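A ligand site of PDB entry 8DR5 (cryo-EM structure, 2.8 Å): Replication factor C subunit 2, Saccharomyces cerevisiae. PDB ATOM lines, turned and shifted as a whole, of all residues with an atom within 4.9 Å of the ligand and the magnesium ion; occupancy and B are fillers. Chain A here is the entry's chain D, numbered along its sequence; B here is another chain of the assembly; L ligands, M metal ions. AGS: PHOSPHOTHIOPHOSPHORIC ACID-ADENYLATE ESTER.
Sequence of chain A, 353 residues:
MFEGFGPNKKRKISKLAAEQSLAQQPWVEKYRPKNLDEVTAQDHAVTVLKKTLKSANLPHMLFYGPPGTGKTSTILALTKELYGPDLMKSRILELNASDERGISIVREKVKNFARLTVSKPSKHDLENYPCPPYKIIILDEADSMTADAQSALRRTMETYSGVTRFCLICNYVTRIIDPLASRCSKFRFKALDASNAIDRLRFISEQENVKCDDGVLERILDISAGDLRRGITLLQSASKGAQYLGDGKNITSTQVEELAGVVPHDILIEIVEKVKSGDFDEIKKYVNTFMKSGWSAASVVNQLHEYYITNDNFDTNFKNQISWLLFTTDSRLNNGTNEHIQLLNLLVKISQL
OG1 of Thr 72 is bound to the magnesium ion, at 2.2 Å.
O2G of the ligand is bound to the magnesium ion, at 2.3 Å.
OD2 of Asp 140 touches the magnesium ion, 3.7 Å away.
Arg 184 of chain B touches the magnesium ion.
The nearest printed residue that does not touch the magnesium ion is Glu 159 of chain B (4.1 Å).
The guanidinium group of Arg 155 of chain B lies within hydrogen-bond range of the side-chain amide oxygen of Asn 171.
NZ of Lys 71 sits at hydrogen-bond distance from O of Pro 66 (3.1 Å).
The side-chain hydroxyl of Ser 73 sits at hydrogen-bond distance from the guanidinium group of Arg 32, 2.7 Å away.
The side-chain carboxylate (OE2) of Glu 159 of chain B is in salt-bridge range of the guanidinium group (NH2) of Arg 229 (3.2 Å).
NH2 of Arg 184 of chain B lies within salt-bridge range of OE1 of Glu 159 of chain B.
O of Pro 180 of chain B lies close to NH1 of Arg 184 of chain B, 3.5 Å away.
The guanidinium group of Arg 32 lies within salt-bridge range of the side-chain carboxylate of Glu 29 (2.9 Å).
OE2 of Glu 38 is in salt-bridge range of NH1 of Arg 200 (3.7 Å).
N of Thr 72 sits at hydrogen-bond distance from O2B of the ligand.
The guanidinium group (NH2) of Arg 155 of chain B lies close to a sulfur (S1G) of the ligand (3.5 Å).
The backbone NH of Lys 71 lies within hydrogen-bond range of an oxygen (O2B) of the ligand (3.3 Å).
O1B of the ligand lies within salt-bridge range of NZ of Lys 71.
O3' of the ligand is in hydrogen-bond range of O of Val 28 (2.6 Å).
N of Ser 73 sits at hydrogen-bond distance from O1A of the ligand.
An oxygen (O1A) of the ligand lies within hydrogen-bond range of the side-chain hydroxyl (OG) of Ser 73 (2.8 Å).
The guanidinium group of Arg 229 lies within salt-bridge range of an oxygen (O2A) of the ligand (2.9 Å).
N of Gly 70 is in hydrogen-bond range of N7 of the ligand.
The guanidinium group of Arg 184 of chain B sits close to a sulfur (S1G) of the ligand.
N of Thr 69 sits at hydrogen-bond distance from O1B of the ligand (3.2 Å).
O3G of the ligand lies within hydrogen-bond range of ND2 of Asn 171 (3.2 Å).
O of Tyr 31 sits at hydrogen-bond distance from O2' of the ligand, at 3.2 Å.
The guanidinium group of Arg 32 is in salt-bridge range of an oxygen (O1A) of the ligand, at 3.5 Å.
O1B of the ligand sits at hydrogen-bond distance from N of Gly 68, at 3.5 Å.
OE2 of Glu 159 of chain B sits close to O2A of the ligand, at 3.3 Å.
Merely in contact with the ligand: Thr 40 (3.6 Å), Pro 33 (3.6 Å), Ile 232 (3.6 Å), Leu 228 (3.6 Å), Pro 67 (3.6 Å), Val 39 (3.7 Å), Pro 180 of chain B (3.7 Å), Glu 38 (3.8 Å) and Leu 192 (3.9 Å).
Hydrophobic or aromatic side chains within 4 Å of the ligand: Pro 33, Val 39, Pro 67, Leu 192, Leu 228, Ile 232 and Pro 180 of chain B.
23 residues have an atom within 4 Å of the ligand: Val 28, Tyr 31, Arg 32, Pro 33, Glu 38, Val 39, Thr 40, Pro 67, Gly 68, Thr 69, Gly 70, Lys 71, Thr 72, Ser 73, Asn 171, Leu 192, Leu 228, Arg 229, Ile 232, Arg 155 of chain B, Glu 159 of chain B, Pro 180 of chain B and Arg 184 of chain B.
The nearest printed residue that does not touch the ligand is Pro 66 (4.1 Å).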
ATOM      1  N   TRP A  27     -19.812  32.290  27.079  1.00  0.00           N
ATOM      2  CA  TRP A  27     -19.096  33.118  26.127  1.00  0.00           C
ATOM      3  C   TRP A  27     -18.691  32.315  24.894  1.00  0.00           C
ATOM      4  O   TRP A  27     -18.623  32.864  23.788  1.00  0.00           O
ATOM      5  CB  TRP A  27     -17.860  33.719  26.789  1.00  0.00           C
ATOM      6  CG  TRP A  27     -18.175  34.757  27.819  1.00  0.00           C
ATOM      7  CD1 TRP A  27     -19.412  35.070  28.303  1.00  0.00           C
ATOM      8  CD2 TRP A  27     -17.248  35.599  28.510  1.00  0.00           C
ATOM      9  NE1 TRP A  27     -19.309  36.059  29.256  1.00  0.00           N
ATOM     10  CE2 TRP A  27     -17.995  36.392  29.401  1.00  0.00           C
ATOM     11  CE3 TRP A  27     -15.858  35.745  28.471  1.00  0.00           C
ATOM     12  CZ2 TRP A  27     -17.399  37.347  30.235  1.00  0.00           C
ATOM     13  CZ3 TRP A  27     -15.272  36.685  29.297  1.00  0.00           C
ATOM     14  CH2 TRP A  27     -16.038  37.464  30.164  1.00  0.00           C
ATOM     15  N   VAL A  28     -18.423  31.029  25.069  1.00  0.00           N
ATOM     16  CA  VAL A  28     -18.000  30.182  23.945  1.00  0.00           C
ATOM     17  C   VAL A  28     -19.098  30.121  22.900  1.00  0.00           C
ATOM     18  O   VAL A  28     -18.830  30.221  21.697  1.00  0.00           O
ATOM     19  CB  VAL A  28     -17.616  28.781  24.454  1.00  0.00           C
ATOM     20  CG1 VAL A  28     -16.398  28.873  25.369  1.00  0.00           C
ATOM     21  CG2 VAL A  28     -18.783  28.121  25.187  1.00  0.00           C
ATOM     22  N   GLU A  29     -20.346  29.943  23.330  1.00  0.00           N
ATOM     23  CA  GLU A  29     -21.467  29.932  22.389  1.00  0.00           C
ATOM     24  C   GLU A  29     -21.861  31.326  21.952  1.00  0.00           C
ATOM     25  O   GLU A  29     -22.328  31.516  20.821  1.00  0.00           O
ATOM     26  CB  GLU A  29     -22.672  29.225  23.013  1.00  0.00           C
ATOM     27  CG  GLU A  29     -22.469  27.741  23.243  1.00  0.00           C
ATOM     28  CD  GLU A  29     -22.418  26.960  21.940  1.00  0.00           C
ATOM     29  OE1 GLU A  29     -23.262  27.206  21.063  1.00  0.00           O
ATOM     30  OE2 GLU A  29     -21.509  26.114  21.791  1.00  0.00           O
ATOM     31  N   TYR A  31     -19.955  33.913  21.382  1.00  0.00           N
ATOM     32  CA  TYR A  31     -19.007  34.394  20.373  1.00  0.00           C
ATOM     33  C   TYR A  31     -18.723  33.339  19.313  1.00  0.00           C
ATOM     34  O   TYR A  31     -17.627  33.273  18.765  1.00  0.00           O
ATOM     35  CB  TYR A  31     -17.726  34.857  21.041  1.00  0.00           C
ATOM     36  CG  TYR A  31     -17.915  36.026  21.970  1.00  0.00           C
ATOM     37  CD1 TYR A  31     -17.856  35.866  23.345  1.00  0.00           C
ATOM     38  CD2 TYR A  31     -18.142  37.302  21.474  1.00  0.00           C
ATOM     39  CE1 TYR A  31     -18.029  36.934  24.198  1.00  0.00           C
ATOM     40  CE2 TYR A  31     -18.319  38.379  22.317  1.00  0.00           C
ATOM     41  CZ  TYR A  31     -18.255  38.187  23.674  1.00  0.00           C
ATOM     42  OH  TYR A  31     -18.428  39.266  24.508  1.00  0.00           O
ATOM     43  N   ARG A  32     -19.713  32.515  19.003  1.00  0.00           N
ATOM     44  CA  ARG A  32     -19.573  31.562  17.907  1.00  0.00           C
ATOM     45  C   ARG A  32     -19.614  32.303  16.579  1.00  0.00           C
ATOM     46  O   ARG A  32     -20.550  33.084  16.351  1.00  0.00           O
ATOM     47  CB  ARG A  32     -20.669  30.509  17.951  1.00  0.00           C
ATOM     48  CG  ARG A  32     -20.492  29.386  16.951  1.00  0.00           C
ATOM     49  CD  ARG A  32     -21.623  28.379  17.025  1.00  0.00           C
ATOM     50  NE  ARG A  32     -21.437  27.423  18.114  1.00  0.00           N
ATOM     51  CZ  ARG A  32     -20.611  26.389  18.071  1.00  0.00           C
ATOM     52  NH1 ARG A  32     -19.882  26.128  16.998  1.00  0.00           N
ATOM     53  NH2 ARG A  32     -20.520  25.581  19.123  1.00  0.00           N
ATOM     54  N   PRO A  33     -18.622  32.120  15.697  1.00  0.00           N
ATOM     55  CA  PRO A  33     -18.635  32.864  14.427  1.00  0.00           C
ATOM     56  C   PRO A  33     -19.960  32.805  13.699  1.00  0.00           C
ATOM     57  O   PRO A  33     -20.426  31.734  13.306  1.00  0.00           O
ATOM     58  CB  PRO A  33     -17.521  32.181  13.614  1.00  0.00           C
ATOM     59  CG  PRO A  33     -16.575  31.682  14.637  1.00  0.00           C
ATOM     60  CD  PRO A  33     -17.410  31.300  15.833  1.00  0.00           C
ATOM     61  N   GLU A  38     -15.860  35.760  10.492  1.00  0.00           N
ATOM     62  CA  GLU A  38     -15.526  35.714  11.905  1.00  0.00           C
ATOM     63  C   GLU A  38     -14.620  34.539  12.264  1.00  0.00           C
ATOM     64  O   GLU A  38     -14.283  34.375  13.433  1.00  0.00           O
ATOM     65  CB  GLU A  38     -16.800  35.657  12.747  1.00  0.00           C
ATOM     66  CG  GLU A  38     -17.559  36.980  12.805  1.00  0.00           C
ATOM     67  CD  GLU A  38     -18.546  37.031  13.947  1.00  0.00           C
ATOM     68  OE1 GLU A  38     -19.288  36.045  14.140  1.00  0.00           O
ATOM     69  OE2 GLU A  38     -18.586  38.063  14.658  1.00  0.00           O
ATOM     70  N   VAL A  39     -14.245  33.723  11.284  1.00  0.00           N
ATOM     71  CA  VAL A  39     -13.273  32.657  11.509  1.00  0.00           C
ATOM     72  C   VAL A  39     -11.876  33.272  11.471  1.00  0.00           C
ATOM     73  O   VAL A  39     -11.512  33.944  10.504  1.00  0.00           O
ATOM     74  CB  VAL A  39     -13.429  31.541  10.466  1.00  0.00           C
ATOM     75  CG1 VAL A  39     -12.328  30.490  10.628  1.00  0.00           C
ATOM     76  CG2 VAL A  39     -14.804  30.894  10.583  1.00  0.00           C
ATOM     77  N   THR A  40     -11.092  33.035  12.526  1.00  0.00           N
ATOM     78  CA  THR A  40      -9.896  33.835  12.752  1.00  0.00           C
ATOM     79  C   THR A  40      -8.691  33.337  11.948  1.00  0.00           C
ATOM     80  O   THR A  40      -8.087  34.095  11.186  1.00  0.00           O
ATOM     81  CB  THR A  40      -9.569  33.889  14.255  1.00  0.00           C
ATOM     82  OG1 THR A  40      -8.420  34.720  14.457  1.00  0.00           O
ATOM     83  CG2 THR A  40      -9.292  32.500  14.822  1.00  0.00           C
ATOM     84  N   ALA A  41      -8.332  32.064  12.110  1.00  0.00           N
ATOM     85  CA  ALA A  41      -7.052  31.557  11.617  1.00  0.00           C
ATOM     86  C   ALA A  41      -7.245  30.284  10.809  1.00  0.00           C
ATOM     87  O   ALA A  41      -6.528  29.287  10.974  1.00  0.00           O
ATOM     88  CB  ALA A  41      -6.096  31.307  12.777  1.00  0.00           C
ATOM     89  N   GLN A  42      -8.215  30.292   9.893  1.00  0.00           N
ATOM     90  CA  GLN A  42      -8.455  29.178   8.994  1.00  0.00           C
ATOM     91  C   GLN A  42      -8.704  29.694   7.583  1.00  0.00           C
ATOM     92  O   GLN A  42      -9.598  29.220   6.879  1.00  0.00           O
ATOM     93  CB  GLN A  42      -9.619  28.313   9.472  1.00  0.00           C
ATOM     94  CG  GLN A  42      -9.564  27.931  10.945  1.00  0.00           C
ATOM     95  CD  GLN A  42      -8.441  26.948  11.246  1.00  0.00           C
ATOM     96  OE1 GLN A  42      -7.671  26.581  10.365  1.00  0.00           O
ATOM     97  NE2 GLN A  42      -8.355  26.522  12.497  1.00  0.00           N
ATOM     98  N   GLY A  65      -9.168  18.207  12.310  1.00  0.00           N
ATOM     99  CA  GLY A  65      -8.257  19.007  13.096  1.00  0.00           C
ATOM    100  C   GLY A  65      -8.423  18.754  14.573  1.00  0.00           C
ATOM    101  O   GLY A  65      -9.278  17.974  15.006  1.00  0.00           O
ATOM    102  N   PRO A  66      -7.605  19.413  15.393  1.00  0.00           N
ATOM    103  CA  PRO A  66      -7.696  19.231  16.843  1.00  0.00           C
ATOM    104  C   PRO A  66      -8.910  19.928  17.414  1.00  0.00           C
ATOM    105  O   PRO A  66      -9.573  20.721  16.714  1.00  0.00           O
ATOM    106  CB  PRO A  66      -6.393  19.842  17.358  1.00  0.00           C
ATOM    107  CG  PRO A  66      -5.986  20.827  16.322  1.00  0.00           C
ATOM    108  CD  PRO A  66      -6.514  20.327  15.008  1.00  0.00           C
ATOM    109  N   PRO A  67      -9.246  19.678  18.683  1.00  0.00           N
ATOM    110  CA  PRO A  67     -10.475  20.256  19.250  1.00  0.00           C
ATOM    111  C   PRO A  67     -10.424  21.781  19.288  1.00  0.00           C
ATOM    112  O   PRO A  67      -9.372  22.390  19.435  1.00  0.00           O
ATOM    113  CB  PRO A  67     -10.515  19.667  20.661  1.00  0.00           C
ATOM    114  CG  PRO A  67      -9.661  18.451  20.605  1.00  0.00           C
ATOM    115  CD  PRO A  67      -8.579  18.764  19.622  1.00  0.00           C
ATOM    116  N   GLY A  68     -11.599  22.382  19.145  1.00  0.00           N
ATOM    117  CA  GLY A  68     -11.750  23.821  19.319  1.00  0.00           C
ATOM    118  C   GLY A  68     -11.046  24.655  18.273  1.00  0.00           C
ATOM    119  O   GLY A  68     -10.514  25.723  18.593  1.00  0.00           O
ATOM    120  N   THR A  69     -11.030  24.189  17.015  1.00  0.00           N
ATOM    121  CA  THR A  69     -10.429  24.943  15.925  1.00  0.00           C
ATOM    122  C   THR A  69     -11.455  25.606  15.010  1.00  0.00           C
ATOM    123  O   THR A  69     -11.058  26.334  14.094  1.00  0.00           O
ATOM    124  CB  THR A  69      -9.532  24.026  15.080  1.00  0.00           C
ATOM    125  OG1 THR A  69     -10.285  22.911  14.606  1.00  0.00           O
ATOM    126  CG2 THR A  69      -8.356  23.532  15.913  1.00  0.00           C
ATOM    127  N   GLY A  70     -12.745  25.381  15.241  1.00  0.00           N
ATOM    128  CA  GLY A  70     -13.787  26.050  14.478  1.00  0.00           C
ATOM    129  C   GLY A  70     -14.201  25.330  13.213  1.00  0.00           C
ATOM    130  O   GLY A  70     -14.230  25.928  12.133  1.00  0.00           O
ATOM    131  N   LYS A  71     -14.530  24.043  13.339  1.00  0.00           N
ATOM    132  CA  LYS A  71     -15.021  23.263  12.204  1.00  0.00           C
ATOM    133  C   LYS A  71     -16.541  23.295  12.121  1.00  0.00           C
ATOM    134  O   LYS A  71     -17.104  23.615  11.061  1.00  0.00           O
ATOM    135  CB  LYS A  71     -14.525  21.822  12.315  1.00  0.00           C
ATOM    136  CG  LYS A  71     -13.022  21.682  12.497  1.00  0.00           C
ATOM    137  CD  LYS A  71     -12.573  20.229  12.494  1.00  0.00           C
ATOM    138  CE  LYS A  71     -12.847  19.549  13.824  1.00  0.00           C
ATOM    139  NZ  LYS A  71     -12.025  20.100  14.932  1.00  0.00           N
ATOM    140  N   THR A  72     -17.215  22.977  13.224  1.00  0.00           N
ATOM    141  CA  THR A  72     -18.669  23.081  13.267  1.00  0.00           C
ATOM    142  C   THR A  72     -19.113  24.509  12.997  1.00  0.00           C
ATOM    143  O   THR A  72     -20.071  24.747  12.248  1.00  0.00           O
ATOM    144  CB  THR A  72     -19.203  22.602  14.615  1.00  0.00           C
ATOM    145  OG1 THR A  72     -18.375  21.528  15.100  1.00  0.00           O
ATOM    146  CG2 THR A  72     -20.637  22.119  14.480  1.00  0.00           C
ATOM    147  N   SER A  73     -18.429  25.477  13.603  1.00  0.00           N
ATOM    148  CA  SER A  73     -18.755  26.881  13.355  1.00  0.00           C
ATOM    149  C   SER A  73     -18.564  27.217  11.888  1.00  0.00           C
ATOM    150  O   SER A  73     -19.393  27.929  11.297  1.00  0.00           O
ATOM    151  CB  SER A  73     -17.875  27.783  14.232  1.00  0.00           C
ATOM    152  OG  SER A  73     -18.046  27.491  15.596  1.00  0.00           O
ATOM    153  N   ASP A 140     -21.425  15.150  11.446  1.00  0.00           N
ATOM    154  CA  ASP A 140     -20.476  15.629  12.434  1.00  0.00           C
ATOM    155  C   ASP A 140     -20.025  14.491  13.322  1.00  0.00           C
ATOM    156  O   ASP A 140     -20.762  13.531  13.580  1.00  0.00           O
ATOM    157  CB  ASP A 140     -21.097  16.750  13.274  1.00  0.00           C
ATOM    158  CG  ASP A 140     -20.052  17.655  13.898  1.00  0.00           C
ATOM    159  OD1 ASP A 140     -18.856  17.315  13.827  1.00  0.00           O
ATOM    160  OD2 ASP A 140     -20.426  18.697  14.466  1.00  0.00           O
ATOM    161  N   GLU A 141     -18.786  14.587  13.820  1.00  0.00           N
ATOM    162  CA  GLU A 141     -18.183  13.536  14.629  1.00  0.00           C
ATOM    163  C   GLU A 141     -18.206  12.199  13.878  1.00  0.00           C
ATOM    164  O   GLU A 141     -18.518  11.146  14.444  1.00  0.00           O
ATOM    165  CB  GLU A 141     -18.881  13.411  15.986  1.00  0.00           C
ATOM    166  CG  GLU A 141     -18.531  14.536  16.948  1.00  0.00           C
ATOM    167  CD  GLU A 141     -19.743  15.171  17.582  1.00  0.00           C
ATOM    168  OE1 GLU A 141     -20.763  14.473  17.774  1.00  0.00           O
ATOM    169  OE2 GLU A 141     -19.683  16.379  17.900  1.00  0.00           O
ATOM    170  N   ASN A 171     -12.237  14.553  14.281  1.00  0.00           N
ATOM    171  CA  ASN A 171     -11.018  14.900  14.994  1.00  0.00           C
ATOM    172  C   ASN A 171      -9.841  14.005  14.636  1.00  0.00           C
ATOM    173  O   ASN A 171      -8.698  14.464  14.660  1.00  0.00           O
ATOM    174  CB  ASN A 171     -11.244  14.828  16.503  1.00  0.00           C
ATOM    175  CG  ASN A 171     -11.805  16.109  17.074  1.00  0.00           C
ATOM    176  OD1 ASN A 171     -12.867  16.110  17.699  1.00  0.00           O
ATOM    177  ND2 ASN A 171     -11.094  17.216  16.865  1.00  0.00           N
ATOM    178  N   LEU A 192      -4.803  26.779  17.109  1.00  0.00           N
ATOM    179  CA  LEU A 192      -4.951  28.202  17.382  1.00  0.00           C
ATOM    180  C   LEU A 192      -4.028  28.582  18.534  1.00  0.00           C
ATOM    181  O   LEU A 192      -4.169  28.075  19.653  1.00  0.00           O
ATOM    182  CB  LEU A 192      -6.406  28.539  17.720  1.00  0.00           C
ATOM    183  CG  LEU A 192      -7.426  28.069  16.681  1.00  0.00           C
ATOM    184  CD1 LEU A 192      -8.837  28.381  17.134  1.00  0.00           C
ATOM    185  CD2 LEU A 192      -7.150  28.695  15.327  1.00  0.00           C
ATOM    186  N   ARG A 200      -8.853  37.653  18.060  1.00  0.00           N
ATOM    187  CA  ARG A 200     -10.206  37.283  18.461  1.00  0.00           C
ATOM    188  C   ARG A 200     -10.371  37.340  19.975  1.00  0.00           C
ATOM    189  O   ARG A 200     -11.388  37.839  20.479  1.00  0.00           O
ATOM    190  CB  ARG A 200     -10.544  35.889  17.928  1.00  0.00           C
ATOM    191  CG  ARG A 200     -11.967  35.435  18.232  1.00  0.00           C
ATOM    192  CD  ARG A 200     -12.993  36.234  17.454  1.00  0.00           C
ATOM    193  NE  ARG A 200     -14.360  35.815  17.746  1.00  0.00           N
ATOM    194  CZ  ARG A 200     -15.439  36.308  17.157  1.00  0.00           C
ATOM    195  NH1 ARG A 200     -15.358  37.258  16.239  1.00  0.00           N
ATOM    196  NH2 ARG A 200     -16.639  35.839  17.509  1.00  0.00           N
ATOM    197  N   LEU A 228      -9.138  27.246  21.273  1.00  0.00           N
ATOM    198  CA  LEU A 228      -9.659  28.588  21.541  1.00  0.00           C
ATOM    199  C   LEU A 228     -10.884  28.545  22.442  1.00  0.00           C
ATOM    200  O   LEU A 228     -11.125  29.510  23.182  1.00  0.00           O
ATOM    201  CB  LEU A 228      -9.988  29.296  20.235  1.00  0.00           C
ATOM    202  CG  LEU A 228     -10.424  30.759  20.324  1.00  0.00           C
ATOM    203  CD1 LEU A 228      -9.476  31.566  21.195  1.00  0.00           C
ATOM    204  CD2 LEU A 228     -10.524  31.374  18.937  1.00  0.00           C
ATOM    205  N   ARG A 229     -11.655  27.454  22.404  1.00  0.00           N
ATOM    206  CA  ARG A 229     -12.769  27.313  23.328  1.00  0.00           C
ATOM    207  C   ARG A 229     -12.282  27.306  24.773  1.00  0.00           C
ATOM    208  O   ARG A 229     -12.869  27.967  25.642  1.00  0.00           O
ATOM    209  CB  ARG A 229     -13.545  26.034  23.015  1.00  0.00           C
ATOM    210  CG  ARG A 229     -14.893  25.922  23.710  1.00  0.00           C
ATOM    211  CD  ARG A 229     -15.334  24.473  23.880  1.00  0.00           C
ATOM    212  NE  ARG A 229     -16.033  23.959  22.701  1.00  0.00           N
ATOM    213  CZ  ARG A 229     -15.487  23.192  21.764  1.00  0.00           C
ATOM    214  NH1 ARG A 229     -14.214  22.807  21.827  1.00  0.00           N
ATOM    215  NH2 ARG A 229     -16.225  22.789  20.742  1.00  0.00           N
ATOM    216  N   ILE A 232     -11.297  30.859  25.758  1.00  0.00           N
ATOM    217  CA  ILE A 232     -12.454  31.706  26.034  1.00  0.00           C
ATOM    218  C   ILE A 232     -13.053  31.359  27.387  1.00  0.00           C
ATOM    219  O   ILE A 232     -13.449  32.236  28.161  1.00  0.00           O
ATOM    220  CB  ILE A 232     -13.495  31.591  24.899  1.00  0.00           C
ATOM    221  CG1 ILE A 232     -12.929  32.177  23.605  1.00  0.00           C
ATOM    222  CG2 ILE A 232     -14.782  32.305  25.286  1.00  0.00           C
ATOM    223  CD1 ILE A 232     -13.680  31.743  22.367  1.00  0.00           C
ATOM    224  N   ARG B 155     -21.313  15.821  23.258  1.00  0.00           N
ATOM    225  CA  ARG B 155     -20.680  17.008  22.710  1.00  0.00           C
ATOM    226  C   ARG B 155     -21.714  17.980  22.153  1.00  0.00           C
ATOM    227  O   ARG B 155     -21.870  19.108  22.637  1.00  0.00           O
ATOM    228  CB  ARG B 155     -19.673  16.606  21.632  1.00  0.00           C
ATOM    229  CG  ARG B 155     -18.516  15.775  22.190  1.00  0.00           C
ATOM    230  CD  ARG B 155     -17.743  15.057  21.107  1.00  0.00           C
ATOM    231  NE  ARG B 155     -17.221  15.985  20.107  1.00  0.00           N
ATOM    232  CZ  ARG B 155     -16.287  15.676  19.211  1.00  0.00           C
ATOM    233  NH1 ARG B 155     -15.742  14.467  19.179  1.00  0.00           N
ATOM    234  NH2 ARG B 155     -15.890  16.600  18.346  1.00  0.00           N
ATOM    235  N   GLU B 159     -23.362  21.586  23.247  1.00  0.00           N
ATOM    236  CA  GLU B 159     -23.125  22.734  22.382  1.00  0.00           C
ATOM    237  C   GLU B 159     -24.390  23.287  21.738  1.00  0.00           C
ATOM    238  O   GLU B 159     -24.335  24.371  21.158  1.00  0.00           O
ATOM    239  CB  GLU B 159     -22.116  22.364  21.290  1.00  0.00           C
ATOM    240  CG  GLU B 159     -20.679  22.342  21.766  1.00  0.00           C
ATOM    241  CD  GLU B 159     -19.701  22.775  20.690  1.00  0.00           C
ATOM    242  OE1 GLU B 159     -19.462  21.993  19.739  1.00  0.00           O
ATOM    243  OE2 GLU B 159     -19.175  23.902  20.788  1.00  0.00           O
ATOM    244  N   PRO B 180     -12.320  16.424  23.752  1.00  0.00           N
ATOM    245  CA  PRO B 180     -13.434  17.355  23.463  1.00  0.00           C
ATOM    246  C   PRO B 180     -14.273  17.685  24.686  1.00  0.00           C
ATOM    247  O   PRO B 180     -14.658  18.848  24.876  1.00  0.00           O
ATOM    248  CB  PRO B 180     -14.244  16.602  22.397  1.00  0.00           C
ATOM    249  CG  PRO B 180     -13.263  15.671  21.764  1.00  0.00           C
ATOM    250  CD  PRO B 180     -12.351  15.248  22.860  1.00  0.00           C
ATOM    251  N   ARG B 184     -14.953  21.262  26.520  1.00  0.00           N
ATOM    252  CA  ARG B 184     -16.288  21.827  26.612  1.00  0.00           C
ATOM    253  C   ARG B 184     -16.712  22.200  28.027  1.00  0.00           C
ATOM    254  O   ARG B 184     -17.834  22.668  28.209  1.00  0.00           O
ATOM    255  CB  ARG B 184     -17.309  20.847  26.023  1.00  0.00           C
ATOM    256  CG  ARG B 184     -17.317  20.785  24.511  1.00  0.00           C
ATOM    257  CD  ARG B 184     -18.173  19.631  24.017  1.00  0.00           C
ATOM    258  NE  ARG B 184     -18.480  19.758  22.592  1.00  0.00           N
ATOM    259  CZ  ARG B 184     -17.621  19.477  21.615  1.00  0.00           C
ATOM    260  NH1 ARG B 184     -16.390  19.064  21.877  1.00  0.00           N
ATOM    261  NH2 ARG B 184     -18.007  19.632  20.354  1.00  0.00           N
HETATM  262  PG  AGS L   1     -14.627  19.774  18.075  1.00  0.00           P
HETATM  263  S1G AGS L   1     -14.035  19.233  19.819  1.00  0.00           S
HETATM  264  O2G AGS L   1     -16.044  18.973  17.685  1.00  0.00           O
HETATM  265  O3G AGS L   1     -13.446  19.410  16.937  1.00  0.00           O
HETATM  266  PB  AGS L   1     -14.679  22.411  16.809  1.00  0.00           P
HETATM  267  O1B AGS L   1     -13.340  22.132  16.166  1.00  0.00           O
HETATM  268  O2B AGS L   1     -15.785  22.198  15.788  1.00  0.00           O
HETATM  269  O3B AGS L   1     -14.913  21.389  18.090  1.00  0.00           O
HETATM  270  PA  AGS L   1     -16.057  24.830  17.511  1.00  0.00           P
HETATM  271  O1A AGS L   1     -16.578  25.180  16.152  1.00  0.00           O
HETATM  272  O2A AGS L   1     -17.102  24.051  18.265  1.00  0.00           O
HETATM  273  O3A AGS L   1     -14.709  23.939  17.374  1.00  0.00           O
HETATM  274  O5' AGS L   1     -15.692  26.220  18.357  1.00  0.00           O
HETATM  275  C5' AGS L   1     -16.083  26.313  19.691  1.00  0.00           C
HETATM  276  C4' AGS L   1     -15.908  27.714  20.166  1.00  0.00           C
HETATM  277  O4' AGS L   1     -14.622  28.015  20.211  1.00  0.00           O
HETATM  278  C3' AGS L   1     -16.622  28.758  19.094  1.00  0.00           C
HETATM  279  O3' AGS L   1     -18.014  29.061  19.541  1.00  0.00           O
HETATM  280  C2' AGS L   1     -15.943  29.796  19.123  1.00  0.00           C
HETATM  281  O2' AGS L   1     -16.392  30.670  20.231  1.00  0.00           O
HETATM  282  C1' AGS L   1     -14.442  29.272  19.406  1.00  0.00           C
HETATM  283  N9  AGS L   1     -13.779  28.983  18.296  1.00  0.00           N
HETATM  284  C8  AGS L   1     -13.256  27.861  17.817  1.00  0.00           C
HETATM  285  N7  AGS L   1     -12.679  28.135  16.648  1.00  0.00           N
HETATM  286  C5  AGS L   1     -12.843  29.432  16.399  1.00  0.00           C
HETATM  287  C6  AGS L   1     -12.447  30.219  15.352  1.00  0.00           C
HETATM  288  N6  AGS L   1     -11.698  29.785  14.164  1.00  0.00           N
HETATM  289  N1  AGS L   1     -12.740  31.508  15.346  1.00  0.00           N
HETATM  290  C2  AGS L   1     -13.426  32.041  16.375  1.00  0.00           C
HETATM  291  N3  AGS L   1     -13.809  31.266  17.408  1.00  0.00           N
HETATM  292  C4  AGS L   1     -13.513  29.964  17.411  1.00  0.00           C
HETATM  293 MG    MG M   1     -17.690  20.087  16.572  1.00  0.00          MG
